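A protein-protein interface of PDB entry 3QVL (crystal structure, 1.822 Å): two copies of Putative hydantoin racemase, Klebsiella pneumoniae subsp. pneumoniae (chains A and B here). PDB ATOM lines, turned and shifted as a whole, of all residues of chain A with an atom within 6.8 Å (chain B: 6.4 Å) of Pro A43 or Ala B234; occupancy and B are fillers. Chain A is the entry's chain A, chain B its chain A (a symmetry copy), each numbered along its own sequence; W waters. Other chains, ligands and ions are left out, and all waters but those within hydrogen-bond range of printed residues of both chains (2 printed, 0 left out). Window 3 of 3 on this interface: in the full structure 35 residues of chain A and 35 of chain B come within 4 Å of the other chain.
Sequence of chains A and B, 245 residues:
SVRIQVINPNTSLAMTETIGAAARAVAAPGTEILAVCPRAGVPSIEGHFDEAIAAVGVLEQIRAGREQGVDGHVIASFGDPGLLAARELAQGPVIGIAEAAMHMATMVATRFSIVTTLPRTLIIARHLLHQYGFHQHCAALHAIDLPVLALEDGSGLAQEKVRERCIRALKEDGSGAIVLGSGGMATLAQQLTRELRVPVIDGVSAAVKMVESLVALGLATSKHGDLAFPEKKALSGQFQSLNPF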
ATOM      1  N   ASN A   8      21.673   3.855   9.604  1.00  0.00           N
ATOM      2  CA  ASN A   8      21.413   4.841   8.567  1.00  0.00           C
ATOM      3  C   ASN A   8      21.023   4.081   7.301  1.00  0.00           C
ATOM      4  O   ASN A   8      21.841   3.347   6.752  1.00  0.00           O
ATOM      5  CB  ASN A   8      22.651   5.712   8.320  1.00  0.00           C
ATOM      6  CG  ASN A   8      22.451   6.723   7.197  1.00  0.00           C
ATOM      7  OD1 ASN A   8      21.323   7.012   6.791  1.00  0.00           O
ATOM      8  ND2 ASN A   8      23.554   7.267   6.691  1.00  0.00           N
ATOM      9  N   ASN A  10      20.469   5.104   4.297  1.00  0.00           N
ATOM     10  CA  ASN A  10      21.238   5.510   3.120  1.00  0.00           C
ATOM     11  C   ASN A  10      22.725   5.180   3.279  1.00  0.00           C
ATOM     12  O   ASN A  10      23.181   4.887   4.386  1.00  0.00           O
ATOM     13  CB  ASN A  10      21.000   6.988   2.762  1.00  0.00           C
ATOM     14  CG  ASN A  10      21.629   7.952   3.753  1.00  0.00           C
ATOM     15  OD1 ASN A  10      22.835   7.918   4.002  1.00  0.00           O
ATOM     16  ND2 ASN A  10      20.810   8.838   4.303  1.00  0.00           N
ATOM     17  N   THR A  11      23.471   5.233   2.177  1.00  0.00           N
ATOM     18  CA  THR A  11      24.869   4.789   2.164  1.00  0.00           C
ATOM     19  C   THR A  11      25.890   5.898   2.434  1.00  0.00           C
ATOM     20  O   THR A  11      27.100   5.658   2.374  1.00  0.00           O
ATOM     21  CB  THR A  11      25.230   4.081   0.836  1.00  0.00           C
ATOM     22  OG1 THR A  11      25.004   4.976  -0.260  1.00  0.00           O
ATOM     23  CG2 THR A  11      24.396   2.820   0.646  1.00  0.00           C
ATOM     24  N   SER A  12      25.408   7.104   2.731  1.00  0.00           N
ATOM     25  CA  SER A  12      26.286   8.229   3.048  1.00  0.00           C
ATOM     26  C   SER A  12      26.966   8.027   4.399  1.00  0.00           C
ATOM     27  O   SER A  12      26.297   7.974   5.435  1.00  0.00           O
ATOM     28  CB  SER A  12      25.501   9.545   3.045  1.00  0.00           C
ATOM     29  OG  SER A  12      26.275  10.609   3.578  1.00  0.00           O
ATOM     30  N   LEU A  13      28.292   7.909   4.382  1.00  0.00           N
ATOM     31  CA  LEU A  13      29.058   7.776   5.620  1.00  0.00           C
ATOM     32  C   LEU A  13      29.008   9.084   6.408  1.00  0.00           C
ATOM     33  O   LEU A  13      28.979   9.070   7.639  1.00  0.00           O
ATOM     34  CB  LEU A  13      30.509   7.365   5.344  1.00  0.00           C
ATOM     35  CG  LEU A  13      31.160   6.357   6.309  1.00  0.00           C
ATOM     36  CD1 LEU A  13      32.530   5.959   5.808  1.00  0.00           C
ATOM     37  CD2 LEU A  13      31.270   6.864   7.746  1.00  0.00           C
ATOM     38  N   MET A  15      26.480  11.187   6.651  1.00  0.00           N
ATOM     39  CA  MET A  15      25.221  11.193   7.399  1.00  0.00           C
ATOM     40  C   MET A  15      25.234  10.160   8.532  1.00  0.00           C
ATOM     41  O   MET A  15      24.671  10.403   9.602  1.00  0.00           O
ATOM     42  CB  MET A  15      24.028  10.989   6.456  1.00  0.00           C
ATOM     43  CG  MET A  15      22.651  11.067   7.123  1.00  0.00           C
ATOM     44  SD  MET A  15      21.405  12.048   6.245  1.00  0.00           S
ATOM     45  CE  MET A  15      21.919  11.875   4.540  1.00  0.00           C
ATOM     46  N   GLY A  41      23.244   0.386  -1.805  1.00  0.00           N
ATOM     47  CA  GLY A  41      22.015   1.166  -1.806  1.00  0.00           C
ATOM     48  C   GLY A  41      22.122   2.546  -2.417  1.00  0.00           C
ATOM     49  O   GLY A  41      22.726   2.732  -3.476  1.00  0.00           O
ATOM     50  N   VAL A  42      21.531   3.514  -1.725  1.00  0.00           N
ATOM     51  CA  VAL A  42      21.376   4.871  -2.229  1.00  0.00           C
ATOM     52  C   VAL A  42      22.023   5.875  -1.256  1.00  0.00           C
ATOM     53  O   VAL A  42      21.867   5.736  -0.044  1.00  0.00           O
ATOM     54  CB  VAL A  42      19.864   5.172  -2.494  1.00  0.00           C
ATOM     55  CG1 VAL A  42      19.055   5.249  -1.191  1.00  0.00           C
ATOM     56  CG2 VAL A  42      19.685   6.415  -3.326  1.00  0.00           C
ATOM     57  N   PRO A  43      22.778   6.865  -1.781  1.00  0.00           N
ATOM     58  CA  PRO A  43      23.466   7.852  -0.933  1.00  0.00           C
ATOM     59  C   PRO A  43      22.532   8.729  -0.092  1.00  0.00           C
ATOM     60  O   PRO A  43      22.909   9.151   1.001  1.00  0.00           O
ATOM     61  CB  PRO A  43      24.232   8.712  -1.945  1.00  0.00           C
ATOM     62  CG  PRO A  43      24.422   7.823  -3.120  1.00  0.00           C
ATOM     63  CD  PRO A  43      23.160   7.020  -3.198  1.00  0.00           C
ATOM     64  N   SER A  44      21.337   9.003  -0.608  1.00  0.00           N
ATOM     65  CA  SER A  44      20.309   9.731   0.138  1.00  0.00           C
ATOM     66  C   SER A  44      18.920   9.293  -0.309  1.00  0.00           C
ATOM     67  O   SER A  44      18.730   8.868  -1.450  1.00  0.00           O
ATOM     68  CB  SER A  44      20.474  11.246  -0.019  1.00  0.00           C
ATOM     69  OG  SER A  44      20.232  11.660  -1.351  1.00  0.00           O
ATOM     70  N   ILE A  45      17.954   9.402   0.597  1.00  0.00           N
ATOM     71  CA  ILE A  45      16.593   8.951   0.331  1.00  0.00           C
ATOM     72  C   ILE A  45      15.683  10.147   0.053  1.00  0.00           C
ATOM     73  O   ILE A  45      15.386  10.941   0.950  1.00  0.00           O
ATOM     74  CB  ILE A  45      16.051   8.079   1.485  1.00  0.00           C
ATOM     75  CG1 ILE A  45      17.000   6.904   1.747  1.00  0.00           C
ATOM     76  CG2 ILE A  45      14.657   7.563   1.155  1.00  0.00           C
ATOM     77  CD1 ILE A  45      17.012   6.424   3.180  1.00  0.00           C
ATOM     78  N   VAL A 148      18.813  16.439   0.202  1.00  0.00           N
ATOM     79  CA  VAL A 148      19.077  15.862   1.522  1.00  0.00           C
ATOM     80  C   VAL A 148      20.542  16.025   1.951  1.00  0.00           C
ATOM     81  O   VAL A 148      20.825  16.396   3.094  1.00  0.00           O
ATOM     82  CB  VAL A 148      18.640  14.370   1.572  1.00  0.00           C
ATOM     83  CG1 VAL A 148      19.239  13.651   2.772  1.00  0.00           C
ATOM     84  CG2 VAL A 148      17.121  14.269   1.596  1.00  0.00           C
ATOM     85  N   LEU A 149      21.461  15.781   1.021  1.00  0.00           N
ATOM     86  CA  LEU A 149      22.895  15.819   1.313  1.00  0.00           C
ATOM     87  C   LEU A 149      23.478  17.227   1.482  1.00  0.00           C
ATOM     88  O   LEU A 149      24.653  17.373   1.831  1.00  0.00           O
ATOM     89  CB  LEU A 149      23.682  15.022   0.264  1.00  0.00           C
ATOM     90  CG  LEU A 149      23.432  13.508   0.244  1.00  0.00           C
ATOM     91  CD1 LEU A 149      24.102  12.863  -0.954  1.00  0.00           C
ATOM     92  CD2 LEU A 149      23.892  12.845   1.540  1.00  0.00           C
ATOM     93  N   GLU B 231      15.464  11.131  -8.232  1.00  0.00           N
ATOM     94  CA  GLU B 231      16.576  12.076  -8.328  1.00  0.00           C
ATOM     95  C   GLU B 231      17.832  11.345  -8.795  1.00  0.00           C
ATOM     96  O   GLU B 231      18.092  10.218  -8.368  1.00  0.00           O
ATOM     97  CB  GLU B 231      16.832  12.766  -6.983  1.00  0.00           C
ATOM     98  CG  GLU B 231      15.623  13.499  -6.390  1.00  0.00           C
ATOM     99  CD  GLU B 231      15.118  14.643  -7.258  1.00  0.00           C
ATOM    100  OE1 GLU B 231      15.948  15.382  -7.834  1.00  0.00           O
ATOM    101  OE2 GLU B 231      13.885  14.806  -7.358  1.00  0.00           O
ATOM    102  N   LYS B 232      18.592  11.983  -9.682  1.00  0.00           N
ATOM    103  CA  LYS B 232      19.786  11.370 -10.263  1.00  0.00           C
ATOM    104  C   LYS B 232      20.854  11.109  -9.207  1.00  0.00           C
ATOM    105  O   LYS B 232      21.381  12.041  -8.595  1.00  0.00           O
ATOM    106  CB  LYS B 232      20.352  12.231 -11.397  1.00  0.00           C
ATOM    107  CG  LYS B 232      21.508  11.580 -12.148  1.00  0.00           C
ATOM    108  CD  LYS B 232      22.074  12.499 -13.219  1.00  0.00           C
ATOM    109  CE  LYS B 232      23.191  11.819 -14.000  1.00  0.00           C
ATOM    110  NZ  LYS B 232      24.428  11.627 -13.188  1.00  0.00           N
ATOM    111  N   LYS B 233      21.157   9.831  -8.998  1.00  0.00           N
ATOM    112  CA  LYS B 233      22.173   9.416  -8.031  1.00  0.00           C
ATOM    113  C   LYS B 233      22.710   8.021  -8.335  1.00  0.00           C
ATOM    114  O   LYS B 233      22.057   7.223  -9.013  1.00  0.00           O
ATOM    115  CB  LYS B 233      21.633   9.489  -6.597  1.00  0.00           C
ATOM    116  CG  LYS B 233      20.365   8.686  -6.352  1.00  0.00           C
ATOM    117  CD  LYS B 233      19.741   9.033  -5.011  1.00  0.00           C
ATOM    118  CE  LYS B 233      18.844  10.253  -5.086  1.00  0.00           C
ATOM    119  NZ  LYS B 233      18.233  10.541  -3.761  1.00  0.00           N
ATOM    120  N   ALA B 234      23.903   7.740  -7.821  1.00  0.00           N
ATOM    121  CA  ALA B 234      24.573   6.470  -8.057  1.00  0.00           C
ATOM    122  C   ALA B 234      24.059   5.385  -7.121  1.00  0.00           C
ATOM    123  O   ALA B 234      24.135   5.515  -5.899  1.00  0.00           O
ATOM    124  CB  ALA B 234      26.067   6.635  -7.905  1.00  0.00           C
ATOM    125  N   LEU B 235      23.531   4.316  -7.709  1.00  0.00           N
ATOM    126  CA  LEU B 235      23.085   3.154  -6.950  1.00  0.00           C
ATOM    127  C   LEU B 235      24.219   2.136  -6.888  1.00  0.00           C
ATOM    128  O   LEU B 235      24.870   1.864  -7.898  1.00  0.00           O
ATOM    129  CB  LEU B 235      21.828   2.545  -7.581  1.00  0.00           C
ATOM    130  CG  LEU B 235      20.636   3.484  -7.824  1.00  0.00           C
ATOM    131  CD1 LEU B 235      19.541   2.785  -8.617  1.00  0.00           C
ATOM    132  CD2 LEU B 235      20.079   4.047  -6.520  1.00  0.00           C
ATOM    133  N   SER B 236      24.463   1.587  -5.700  1.00  0.00           N
ATOM    134  CA  SER B 236      25.596   0.687  -5.485  1.00  0.00           C
ATOM    135  C   SER B 236      25.185  -0.776  -5.336  1.00  0.00           C
ATOM    136  O   SER B 236      24.041  -1.080  -4.988  1.00  0.00           O
ATOM    137  CB  SER B 236      26.417   1.136  -4.272  1.00  0.00           C
ATOM    138  OG  SER B 236      25.626   1.170  -3.098  1.00  0.00           O
HETATM  139  O   HOH W   1      25.676   3.901  -2.545  1.00  0.00           O
HETATM  140  O   HOH W   2      21.462  11.670  -3.652  1.00  0.00           O
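Among the printed residues, merely in contact across the chains: Gly A41 with Ala B234 (3.9 Å), Gly A41 with Leu B235 (3.5 Å), Val A42 with Lys B233 (3.1 Å), Val A42 with Leu B235 (3.996 Å) and Pro A43 with Ala B234 (3.2 Å).
Of the printed residues of chain B, Gly A41 touches Ala B234, Leu B235 and Ser B236. Pro A43 touches just one residue of chain B: Ala B234 (3.2 Å). Printed residues of chain A within 4 Å of Lys B233: Val A42 (3.1 Å) and Ser A44 (2.9 Å). Printed residues of chain A within 4 Å of Leu B235: Gly A41 and Val A42.
Water W2 bridges OG of Ser A44 (2.6 Å) and NZ of Lys B233 (3.4 Å). Water W1 lies within hydrogen-bond range of OG1 of Thr A11 (2.6 Å), OG of Ser B236 (2.8 Å) and O of Gly A41 (3.3 Å).
The side-chain amide oxygen (OD1) of Asn A10 lies close to the backbone carbonyl oxygen (O) of Pro A43. N of Thr A11 lies within hydrogen-bond range of O of Val A42 (2.8 Å).
Printed residues of chain B that touch a printed residue of chain A: Lys B233, Ala B234, Leu B235 and Ser B236. Hydrophobic or aromatic side chains of chain B within 4 Å of the printed part of chain A: Leu B235. Among the printed residues, no Asp or Glu carboxylate lies within 4 Å of a Lys or Arg side-chain nitrogen of the other chain.
N of Gly A41 sits at hydrogen-bond distance from OG of Ser B236. NZ of Lys B233 sits at hydrogen-bond distance from O of Ser A44.
No position is printed for both chains.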
